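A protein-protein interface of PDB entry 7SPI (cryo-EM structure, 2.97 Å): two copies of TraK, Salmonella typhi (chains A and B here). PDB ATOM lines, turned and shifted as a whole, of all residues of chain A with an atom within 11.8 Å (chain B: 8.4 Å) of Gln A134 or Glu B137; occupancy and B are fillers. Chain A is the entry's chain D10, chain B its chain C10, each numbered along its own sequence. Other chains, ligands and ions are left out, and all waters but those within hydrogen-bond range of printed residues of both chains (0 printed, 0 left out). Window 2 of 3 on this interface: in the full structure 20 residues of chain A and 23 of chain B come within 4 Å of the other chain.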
ATOM      1  N   TRP A 130     -18.601   4.401 -22.145  1.00  0.00           N
ATOM      2  CA  TRP A 130     -18.568   4.335 -23.587  1.00  0.00           C
ATOM      3  C   TRP A 130     -17.156   4.141 -24.074  1.00  0.00           C
ATOM      4  O   TRP A 130     -16.941   3.846 -25.244  1.00  0.00           O
ATOM      5  CB  TRP A 130     -19.153   5.616 -24.173  1.00  0.00           C
ATOM      6  CG  TRP A 130     -18.662   6.870 -23.526  1.00  0.00           C
ATOM      7  CD1 TRP A 130     -19.128   7.440 -22.379  1.00  0.00           C
ATOM      8  CD2 TRP A 130     -17.619   7.725 -24.000  1.00  0.00           C
ATOM      9  NE1 TRP A 130     -18.431   8.586 -22.102  1.00  0.00           N
ATOM     10  CE2 TRP A 130     -17.501   8.785 -23.084  1.00  0.00           C
ATOM     11  CE3 TRP A 130     -16.770   7.694 -25.108  1.00  0.00           C
ATOM     12  CZ2 TRP A 130     -16.568   9.800 -23.240  1.00  0.00           C
ATOM     13  CZ3 TRP A 130     -15.849   8.700 -25.261  1.00  0.00           C
ATOM     14  CH2 TRP A 130     -15.753   9.741 -24.333  1.00  0.00           C
ATOM     15  N   GLU A 131     -16.183   4.297 -23.182  1.00  0.00           N
ATOM     16  CA  GLU A 131     -14.803   4.219 -23.638  1.00  0.00           C
ATOM     17  C   GLU A 131     -14.457   2.795 -24.056  1.00  0.00           C
ATOM     18  O   GLU A 131     -14.840   1.826 -23.396  1.00  0.00           O
ATOM     19  CB  GLU A 131     -13.856   4.690 -22.539  1.00  0.00           C
ATOM     20  CG  GLU A 131     -14.016   6.154 -22.169  1.00  0.00           C
ATOM     21  CD  GLU A 131     -15.004   6.369 -21.040  1.00  0.00           C
ATOM     22  OE1 GLU A 131     -16.131   5.836 -21.124  1.00  0.00           O
ATOM     23  OE2 GLU A 131     -14.656   7.072 -20.069  1.00  0.00           O
ATOM     24  N   THR A 132     -13.726   2.672 -25.161  1.00  0.00           N
ATOM     25  CA  THR A 132     -13.316   1.381 -25.694  1.00  0.00           C
ATOM     26  C   THR A 132     -11.803   1.353 -25.830  1.00  0.00           C
ATOM     27  O   THR A 132     -11.210   2.286 -26.381  1.00  0.00           O
ATOM     28  CB  THR A 132     -13.973   1.101 -27.050  1.00  0.00           C
ATOM     29  OG1 THR A 132     -13.628   2.142 -27.971  1.00  0.00           O
ATOM     30  CG2 THR A 132     -15.484   1.040 -26.909  1.00  0.00           C
ATOM     31  N   ALA A 133     -11.185   0.287 -25.332  1.00  0.00           N
ATOM     32  CA  ALA A 133      -9.741   0.146 -25.394  1.00  0.00           C
ATOM     33  C   ALA A 133      -9.304  -0.310 -26.784  1.00  0.00           C
ATOM     34  O   ALA A 133     -10.117  -0.702 -27.629  1.00  0.00           O
ATOM     35  CB  ALA A 133      -9.251  -0.836 -24.332  1.00  0.00           C
ATOM     36  N   GLN A 134      -7.997  -0.296 -27.022  1.00  0.00           N
ATOM     37  CA  GLN A 134      -7.475  -0.661 -28.332  1.00  0.00           C
ATOM     38  C   GLN A 134      -7.471  -2.153 -28.523  1.00  0.00           C
ATOM     39  O   GLN A 134      -7.448  -2.899 -27.557  1.00  0.00           O
ATOM     40  CB  GLN A 134      -6.059  -0.128 -28.477  1.00  0.00           C
ATOM     41  CG  GLN A 134      -5.884   1.331 -28.099  1.00  0.00           C
ATOM     42  CD  GLN A 134      -6.089   2.271 -29.269  1.00  0.00           C
ATOM     43  OE1 GLN A 134      -6.772   1.943 -30.237  1.00  0.00           O
ATOM     44  NE2 GLN A 134      -5.492   3.450 -29.183  1.00  0.00           N
ATOM     45  N   ALA A 135      -7.469  -2.600 -29.769  1.00  0.00           N
ATOM     46  CA  ALA A 135      -7.509  -4.027 -30.045  1.00  0.00           C
ATOM     47  C   ALA A 135      -6.298  -4.794 -29.517  1.00  0.00           C
ATOM     48  O   ALA A 135      -6.445  -5.887 -28.990  1.00  0.00           O
ATOM     49  CB  ALA A 135      -7.671  -4.263 -31.528  1.00  0.00           C
ATOM     50  N   TYR A 136      -5.106  -4.239 -29.656  1.00  0.00           N
ATOM     51  CA  TYR A 136      -3.925  -4.895 -29.144  1.00  0.00           C
ATOM     52  C   TYR A 136      -4.006  -5.023 -27.638  1.00  0.00           C
ATOM     53  O   TYR A 136      -3.695  -6.074 -27.084  1.00  0.00           O
ATOM     54  CB  TYR A 136      -2.698  -4.094 -29.554  1.00  0.00           C
ATOM     55  CG  TYR A 136      -1.386  -4.485 -28.919  1.00  0.00           C
ATOM     56  CD1 TYR A 136      -0.718  -5.637 -29.303  1.00  0.00           C
ATOM     57  CD2 TYR A 136      -0.793  -3.671 -27.972  1.00  0.00           C
ATOM     58  CE1 TYR A 136       0.493  -5.980 -28.733  1.00  0.00           C
ATOM     59  CE2 TYR A 136       0.414  -4.003 -27.398  1.00  0.00           C
ATOM     60  CZ  TYR A 136       1.052  -5.155 -27.781  1.00  0.00           C
ATOM     61  OH  TYR A 136       2.253  -5.473 -27.201  1.00  0.00           O
ATOM     62  N   GLU A 137      -4.434  -3.965 -26.965  1.00  0.00           N
ATOM     63  CA  GLU A 137      -4.476  -4.003 -25.519  1.00  0.00           C
ATOM     64  C   GLU A 137      -5.470  -5.021 -25.016  1.00  0.00           C
ATOM     65  O   GLU A 137      -5.190  -5.762 -24.084  1.00  0.00           O
ATOM     66  CB  GLU A 137      -4.768  -2.635 -24.941  1.00  0.00           C
ATOM     67  CG  GLU A 137      -3.587  -1.685 -25.001  1.00  0.00           C
ATOM     68  CD  GLU A 137      -3.842  -0.398 -24.244  1.00  0.00           C
ATOM     69  OE1 GLU A 137      -2.861   0.267 -23.856  1.00  0.00           O
ATOM     70  OE2 GLU A 137      -5.024  -0.055 -24.028  1.00  0.00           O
ATOM     71  N   LYS A 138      -6.628  -5.081 -25.650  1.00  0.00           N
ATOM     72  CA  LYS A 138      -7.641  -6.027 -25.226  1.00  0.00           C
ATOM     73  C   LYS A 138      -7.173  -7.449 -25.435  1.00  0.00           C
ATOM     74  O   LYS A 138      -7.465  -8.319 -24.628  1.00  0.00           O
ATOM     75  CB  LYS A 138      -9.011  -5.745 -25.861  1.00  0.00           C
ATOM     76  CG  LYS A 138      -9.158  -6.071 -27.332  1.00  0.00           C
ATOM     77  CD  LYS A 138     -10.497  -5.578 -27.850  1.00  0.00           C
ATOM     78  CE  LYS A 138     -10.720  -4.127 -27.459  1.00  0.00           C
ATOM     79  NZ  LYS A 138     -11.978  -3.570 -28.023  1.00  0.00           N
ATOM     80  N   LEU A 139      -6.452  -7.693 -26.521  1.00  0.00           N
ATOM     81  CA  LEU A 139      -5.952  -9.027 -26.806  1.00  0.00           C
ATOM     82  C   LEU A 139      -4.992  -9.526 -25.740  1.00  0.00           C
ATOM     83  O   LEU A 139      -5.107 -10.657 -25.278  1.00  0.00           O
ATOM     84  CB  LEU A 139      -5.251  -9.010 -28.158  1.00  0.00           C
ATOM     85  CG  LEU A 139      -4.959 -10.338 -28.844  1.00  0.00           C
ATOM     86  CD1 LEU A 139      -6.238 -11.144 -28.997  1.00  0.00           C
ATOM     87  CD2 LEU A 139      -4.322 -10.070 -30.199  1.00  0.00           C
ATOM     88  N   LEU A 140      -4.066  -8.686 -25.319  1.00  0.00           N
ATOM     89  CA  LEU A 140      -3.160  -9.072 -24.254  1.00  0.00           C
ATOM     90  C   LEU A 140      -3.910  -9.286 -22.962  1.00  0.00           C
ATOM     91  O   LEU A 140      -3.664 -10.253 -22.269  1.00  0.00           O
ATOM     92  CB  LEU A 140      -2.075  -8.019 -24.063  1.00  0.00           C
ATOM     93  CG  LEU A 140      -0.761  -8.111 -24.836  1.00  0.00           C
ATOM     94  CD1 LEU A 140      -0.946  -8.515 -26.289  1.00  0.00           C
ATOM     95  CD2 LEU A 140      -0.038  -6.783 -24.731  1.00  0.00           C
ATOM     96  N   ILE A 141      -4.851  -8.407 -22.648  1.00  0.00           N
ATOM     97  CA  ILE A 141      -5.609  -8.510 -21.404  1.00  0.00           C
ATOM     98  C   ILE A 141      -6.429  -9.784 -21.346  1.00  0.00           C
ATOM     99  O   ILE A 141      -6.461 -10.457 -20.320  1.00  0.00           O
ATOM    100  CB  ILE A 141      -6.534  -7.294 -21.223  1.00  0.00           C
ATOM    101  CG1 ILE A 141      -5.719  -6.058 -20.847  1.00  0.00           C
ATOM    102  CG2 ILE A 141      -7.579  -7.542 -20.146  1.00  0.00           C
ATOM    103  CD1 ILE A 141      -5.028  -6.171 -19.507  1.00  0.00           C
ATOM    104  N   SER A 142      -7.062 -10.146 -22.455  1.00  0.00           N
ATOM    105  CA  SER A 142      -7.881 -11.345 -22.473  1.00  0.00           C
ATOM    106  C   SER A 142      -7.038 -12.571 -22.230  1.00  0.00           C
ATOM    107  O   SER A 142      -7.411 -13.438 -21.450  1.00  0.00           O
ATOM    108  CB  SER A 142      -8.598 -11.480 -23.809  1.00  0.00           C
ATOM    109  OG  SER A 142      -7.684 -11.649 -24.875  1.00  0.00           O
ATOM    110  N   LEU A 143      -5.888 -12.638 -22.881  1.00  0.00           N
ATOM    111  CA  LEU A 143      -5.000 -13.772 -22.706  1.00  0.00           C
ATOM    112  C   LEU A 143      -4.460 -13.858 -21.299  1.00  0.00           C
ATOM    113  O   LEU A 143      -4.363 -14.936 -20.743  1.00  0.00           O
ATOM    114  CB  LEU A 143      -3.859 -13.726 -23.716  1.00  0.00           C
ATOM    115  CG  LEU A 143      -2.770 -14.791 -23.672  1.00  0.00           C
ATOM    116  CD1 LEU A 143      -2.579 -15.382 -25.054  1.00  0.00           C
ATOM    117  CD2 LEU A 143      -1.473 -14.177 -23.176  1.00  0.00           C
ATOM    118  N   ARG A 145      -5.807 -12.861 -18.619  1.00  0.00           N
ATOM    119  CA  ARG A 145      -6.886 -13.360 -17.782  1.00  0.00           C
ATOM    120  C   ARG A 145      -7.114 -14.858 -17.972  1.00  0.00           C
ATOM    121  O   ARG A 145      -7.311 -15.584 -17.000  1.00  0.00           O
ATOM    122  CB  ARG A 145      -8.166 -12.571 -18.056  1.00  0.00           C
ATOM    123  CG  ARG A 145      -9.344 -12.918 -17.166  1.00  0.00           C
ATOM    124  CD  ARG A 145     -10.416 -11.858 -17.312  1.00  0.00           C
ATOM    125  NE  ARG A 145     -10.548 -11.428 -18.700  1.00  0.00           N
ATOM    126  CZ  ARG A 145     -11.326 -10.429 -19.100  1.00  0.00           C
ATOM    127  NH1 ARG A 145     -12.043  -9.753 -18.215  1.00  0.00           N
ATOM    128  NH2 ARG A 145     -11.384 -10.104 -20.385  1.00  0.00           N
ATOM    129  N   GLN B 134     -15.224   5.141 -32.717  1.00  0.00           N
ATOM    130  CA  GLN B 134     -13.788   4.882 -32.598  1.00  0.00           C
ATOM    131  C   GLN B 134     -13.283   4.626 -31.189  1.00  0.00           C
ATOM    132  O   GLN B 134     -14.034   4.774 -30.233  1.00  0.00           O
ATOM    133  CB  GLN B 134     -13.058   6.095 -33.115  1.00  0.00           C
ATOM    134  CG  GLN B 134     -13.525   7.394 -32.504  1.00  0.00           C
ATOM    135  CD  GLN B 134     -12.979   8.586 -33.243  1.00  0.00           C
ATOM    136  OE1 GLN B 134     -11.779   8.685 -33.486  1.00  0.00           O
ATOM    137  NE2 GLN B 134     -13.857   9.500 -33.604  1.00  0.00           N
ATOM    138  N   ALA B 135     -12.011   4.244 -31.053  1.00  0.00           N
ATOM    139  CA  ALA B 135     -11.415   3.993 -29.744  1.00  0.00           C
ATOM    140  C   ALA B 135     -11.140   5.233 -28.971  1.00  0.00           C
ATOM    141  O   ALA B 135     -11.017   6.290 -29.534  1.00  0.00           O
ATOM    142  CB  ALA B 135     -10.148   3.226 -29.882  1.00  0.00           C
ATOM    143  N   TYR B 136     -11.041   5.113 -27.668  1.00  0.00           N
ATOM    144  CA  TYR B 136     -10.845   6.262 -26.828  1.00  0.00           C
ATOM    145  C   TYR B 136      -9.530   6.926 -27.102  1.00  0.00           C
ATOM    146  O   TYR B 136      -9.496   8.116 -27.332  1.00  0.00           O
ATOM    147  CB  TYR B 136     -10.982   5.821 -25.384  1.00  0.00           C
ATOM    148  CG  TYR B 136     -10.681   6.785 -24.283  1.00  0.00           C
ATOM    149  CD1 TYR B 136     -11.615   7.702 -23.845  1.00  0.00           C
ATOM    150  CD2 TYR B 136      -9.494   6.703 -23.615  1.00  0.00           C
ATOM    151  CE1 TYR B 136     -11.331   8.551 -22.798  1.00  0.00           C
ATOM    152  CE2 TYR B 136      -9.202   7.537 -22.578  1.00  0.00           C
ATOM    153  CZ  TYR B 136     -10.119   8.454 -22.171  1.00  0.00           C
ATOM    154  OH  TYR B 136      -9.765   9.248 -21.124  1.00  0.00           O
ATOM    155  N   GLU B 137      -8.428   6.205 -27.103  1.00  0.00           N
ATOM    156  CA  GLU B 137      -7.141   6.870 -27.256  1.00  0.00           C
ATOM    157  C   GLU B 137      -7.018   7.496 -28.614  1.00  0.00           C
ATOM    158  O   GLU B 137      -6.384   8.523 -28.752  1.00  0.00           O
ATOM    159  CB  GLU B 137      -6.000   5.906 -26.983  1.00  0.00           C
ATOM    160  CG  GLU B 137      -6.297   4.866 -25.912  1.00  0.00           C
ATOM    161  CD  GLU B 137      -6.077   5.363 -24.491  1.00  0.00           C
ATOM    162  OE1 GLU B 137      -5.877   4.513 -23.595  1.00  0.00           O
ATOM    163  OE2 GLU B 137      -6.095   6.591 -24.259  1.00  0.00           O
ATOM    164  N   LYS B 138      -7.622   6.898 -29.625  1.00  0.00           N
ATOM    165  CA  LYS B 138      -7.642   7.499 -30.947  1.00  0.00           C
ATOM    166  C   LYS B 138      -8.392   8.806 -30.995  1.00  0.00           C
ATOM    167  O   LYS B 138      -7.921   9.737 -31.615  1.00  0.00           O
ATOM    168  CB  LYS B 138      -8.285   6.546 -31.925  1.00  0.00           C
ATOM    169  CG  LYS B 138      -7.299   5.709 -32.713  1.00  0.00           C
ATOM    170  CD  LYS B 138      -7.994   5.035 -33.880  1.00  0.00           C
ATOM    171  CE  LYS B 138      -8.721   6.052 -34.745  1.00  0.00           C
ATOM    172  NZ  LYS B 138      -7.802   7.072 -35.325  1.00  0.00           N
ATOM    173  N   LEU B 139      -9.543   8.891 -30.337  1.00  0.00           N
ATOM    174  CA  LEU B 139     -10.343  10.106 -30.265  1.00  0.00           C
ATOM    175  C   LEU B 139      -9.629  11.226 -29.570  1.00  0.00           C
ATOM    176  O   LEU B 139      -9.665  12.345 -30.014  1.00  0.00           O
ATOM    177  CB  LEU B 139     -11.624   9.793 -29.518  1.00  0.00           C
ATOM    178  CG  LEU B 139     -12.767  10.765 -29.279  1.00  0.00           C
ATOM    179  CD1 LEU B 139     -13.414  11.173 -30.587  1.00  0.00           C
ATOM    180  CD2 LEU B 139     -13.775  10.056 -28.394  1.00  0.00           C
ATOM    181  N   LEU B 140      -8.961  10.910 -28.466  1.00  0.00           N
ATOM    182  CA  LEU B 140      -8.201  11.920 -27.744  1.00  0.00           C
ATOM    183  C   LEU B 140      -7.140  12.517 -28.653  1.00  0.00           C
ATOM    184  O   LEU B 140      -7.006  13.736 -28.735  1.00  0.00           O
ATOM    185  CB  LEU B 140      -7.534  11.323 -26.507  1.00  0.00           C
ATOM    186  CG  LEU B 140      -8.427  10.765 -25.400  1.00  0.00           C
ATOM    187  CD1 LEU B 140      -7.552  10.309 -24.243  1.00  0.00           C
ATOM    188  CD2 LEU B 140      -9.431  11.806 -24.931  1.00  0.00           C
ATOM    189  N   ILE B 141      -6.388  11.658 -29.338  1.00  0.00           N
ATOM    190  CA  ILE B 141      -5.333  12.137 -30.229  1.00  0.00           C
ATOM    191  C   ILE B 141      -5.907  12.999 -31.313  1.00  0.00           C
ATOM    192  O   ILE B 141      -5.357  14.035 -31.622  1.00  0.00           O
ATOM    193  CB  ILE B 141      -4.577  10.960 -30.853  1.00  0.00           C
ATOM    194  CG1 ILE B 141      -3.696  10.290 -29.802  1.00  0.00           C
ATOM    195  CG2 ILE B 141      -3.705  11.403 -32.015  1.00  0.00           C
ATOM    196  CD1 ILE B 141      -2.748  11.245 -29.115  1.00  0.00           C
ATOM    197  N   SER B 142      -7.037  12.597 -31.867  1.00  0.00           N
ATOM    198  CA  SER B 142      -7.712  13.361 -32.894  1.00  0.00           C
ATOM    199  C   SER B 142      -8.195  14.728 -32.480  1.00  0.00           C
ATOM    200  O   SER B 142      -8.040  15.670 -33.230  1.00  0.00           O
ATOM    201  CB  SER B 142      -8.900  12.560 -33.391  1.00  0.00           C
ATOM    202  OG  SER B 142     -10.027  13.386 -33.564  1.00  0.00           O
ATOM    203  N   LEU B 143      -8.789  14.863 -31.313  1.00  0.00           N
ATOM    204  CA  LEU B 143      -9.204  16.166 -30.843  1.00  0.00           C
ATOM    205  C   LEU B 143      -8.039  17.038 -30.566  1.00  0.00           C
ATOM    206  O   LEU B 143      -8.069  18.213 -30.859  1.00  0.00           O
ATOM    207  CB  LEU B 143     -10.090  16.051 -29.615  1.00  0.00           C
ATOM    208  CG  LEU B 143     -11.594  16.024 -29.878  1.00  0.00           C
ATOM    209  CD1 LEU B 143     -11.940  17.127 -30.860  1.00  0.00           C
ATOM    210  CD2 LEU B 143     -12.048  14.684 -30.424  1.00  0.00           C
ATOM    211  N   ASN B 144      -7.014  16.471 -29.971  1.00  0.00           N
ATOM    212  CA  ASN B 144      -5.813  17.218 -29.668  1.00  0.00           C
ATOM    213  C   ASN B 144      -5.078  17.669 -30.924  1.00  0.00           C
ATOM    214  O   ASN B 144      -4.506  18.739 -30.954  1.00  0.00           O
ATOM    215  CB  ASN B 144      -4.933  16.415 -28.725  1.00  0.00           C
ATOM    216  CG  ASN B 144      -5.246  16.659 -27.272  1.00  0.00           C
ATOM    217  OD1 ASN B 144      -5.409  17.795 -26.841  1.00  0.00           O
ATOM    218  ND2 ASN B 144      -5.306  15.591 -26.503  1.00  0.00           N
ATOM    219  N   ARG B 145      -5.033  16.841 -31.950  1.00  0.00           N
ATOM    220  CA  ARG B 145      -4.425  17.268 -33.188  1.00  0.00           C
ATOM    221  C   ARG B 145      -5.199  18.383 -33.795  1.00  0.00           C
ATOM    222  O   ARG B 145      -4.623  19.365 -34.202  1.00  0.00           O
ATOM    223  CB  ARG B 145      -4.412  16.126 -34.175  1.00  0.00           C
ATOM    224  CG  ARG B 145      -3.654  16.379 -35.457  1.00  0.00           C
ATOM    225  CD  ARG B 145      -3.096  15.067 -35.973  1.00  0.00           C
ATOM    226  NE  ARG B 145      -3.859  13.927 -35.475  1.00  0.00           N
ATOM    227  CZ  ARG B 145      -4.830  13.320 -36.146  1.00  0.00           C
ATOM    228  NH1 ARG B 145      -5.465  12.289 -35.609  1.00  0.00           N
ATOM    229  NH2 ARG B 145      -5.165  13.741 -37.356  1.00  0.00           N
ATOM    230  N   ARG B 213      -9.809  14.938 -18.617  1.00  0.00           N
ATOM    231  CA  ARG B 213      -9.567  13.629 -19.207  1.00  0.00           C
ATOM    232  C   ARG B 213      -8.188  13.497 -19.836  1.00  0.00           C
ATOM    233  O   ARG B 213      -7.619  12.403 -19.825  1.00  0.00           O
ATOM    234  CB  ARG B 213     -10.653  13.351 -20.256  1.00  0.00           C
ATOM    235  CG  ARG B 213     -10.866  11.891 -20.571  1.00  0.00           C
ATOM    236  CD  ARG B 213     -12.319  11.620 -20.921  1.00  0.00           C
ATOM    237  NE  ARG B 213     -13.225  12.110 -19.889  1.00  0.00           N
ATOM    238  CZ  ARG B 213     -14.210  11.397 -19.356  1.00  0.00           C
ATOM    239  NH1 ARG B 213     -14.448  10.154 -19.738  1.00  0.00           N
ATOM    240  NH2 ARG B 213     -14.972  11.948 -18.418  1.00  0.00           N
ATOM    241  N   ALA B 214      -7.633  14.579 -20.378  1.00  0.00           N
ATOM    242  CA  ALA B 214      -6.320  14.539 -21.006  1.00  0.00           C
ATOM    243  C   ALA B 214      -5.728  15.940 -21.026  1.00  0.00           C
ATOM    244  O   ALA B 214      -6.453  16.934 -21.104  1.00  0.00           O
ATOM    245  CB  ALA B 214      -6.390  13.973 -22.428  1.00  0.00           C
ATOM    246  N   ILE B 235      -8.750  18.221 -22.446  1.00  0.00           N
ATOM    247  CA  ILE B 235     -10.000  17.612 -22.859  1.00  0.00           C
ATOM    248  C   ILE B 235     -10.659  17.188 -21.572  1.00  0.00           C
ATOM    249  O   ILE B 235      -9.977  16.753 -20.657  1.00  0.00           O
ATOM    250  CB  ILE B 235      -9.780  16.394 -23.764  1.00  0.00           C
ATOM    251  CG1 ILE B 235      -8.860  16.757 -24.929  1.00  0.00           C
ATOM    252  CG2 ILE B 235     -11.104  15.867 -24.295  1.00  0.00           C
ATOM    253  CD1 ILE B 235      -8.746  15.665 -25.966  1.00  0.00           C
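Of the 15 printed residues of chain B, 6 touch a printed residue of chain A. Hydrophobic or aromatic side chains of chain B within 4 Å of the printed part of chain A: Ala B135, Tyr B136 and Leu B139. Of the 15 printed residues of chain A, 4 touch a printed residue of chain B. Among the printed residues, 8 pairs touch across the chains. Among the printed residues, Asp or Glu carboxylates within 4 Å of a Lys or Arg side-chain nitrogen of the other chain: Glu A131 with Arg B213.
Among the printed residues, merely in contact across the chains: Glu A131 with Tyr B136 (3.3 Å), Gln A134 with Glu B137 (3.3 Å), Thr A132 with Ala B135 (3.4 Å), Gln A134 with Ala B135 (3.6 Å) and Trp A130 with Leu B139 (3.99 Å).
The backbone carbonyl oxygen of Ile B235 is in hydrogen-bond range of the backbone NH of Arg B213.
Of chain B, only Ala B135 (3.6 Å) and Glu B137 (3.3 Å) come within 4 Å of Gln A134. Glu B137 touches just one residue of chain A: Gln A134 (3.3 Å). Ala A133 touches none of the printed residues of chain B. No residue of chain B comes within 4 Å of Ala A135. Of chain A, only Glu A131 and Thr A132 come within 4 Å of Tyr B136. No residue of chain A comes within 4 Å of Lys B138. No residue of chain A comes within 4 Å of Leu B140. No residue of chain A comes within 4 Å of Ile B141. Printed residues of chain B within 4 Å of Trp A130: Leu B139 (3.99 Å). Of the printed residues of chain A, Gln B134 touches Thr A132 (3.5 Å). Of the printed residues of chain A, Arg B213 touches Glu A131. The nearest residue of chain B that does not touch Gln A134 is Lys B138 (4.1 Å). The nearest printed residue of chain B that does not touch Trp A130 is Arg B213 (4.1 Å).
Gln A134 touches Ala B135, but with the chains exchanged Ala A135 does not touch Gln B134 (9.4 Å). Gln A134 touches Glu B137, but with the chains exchanged Glu A137 does not touch Gln B134 (11.9 Å).
O of Gln B134 sits at hydrogen-bond distance from OG1 of Thr A132 (3.5 Å). NH1 of Arg B213 lies within salt-bridge range of OE2 of Glu A131 (3.1 Å). O of Thr A132 sits at hydrogen-bond distance from N of Tyr B136.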
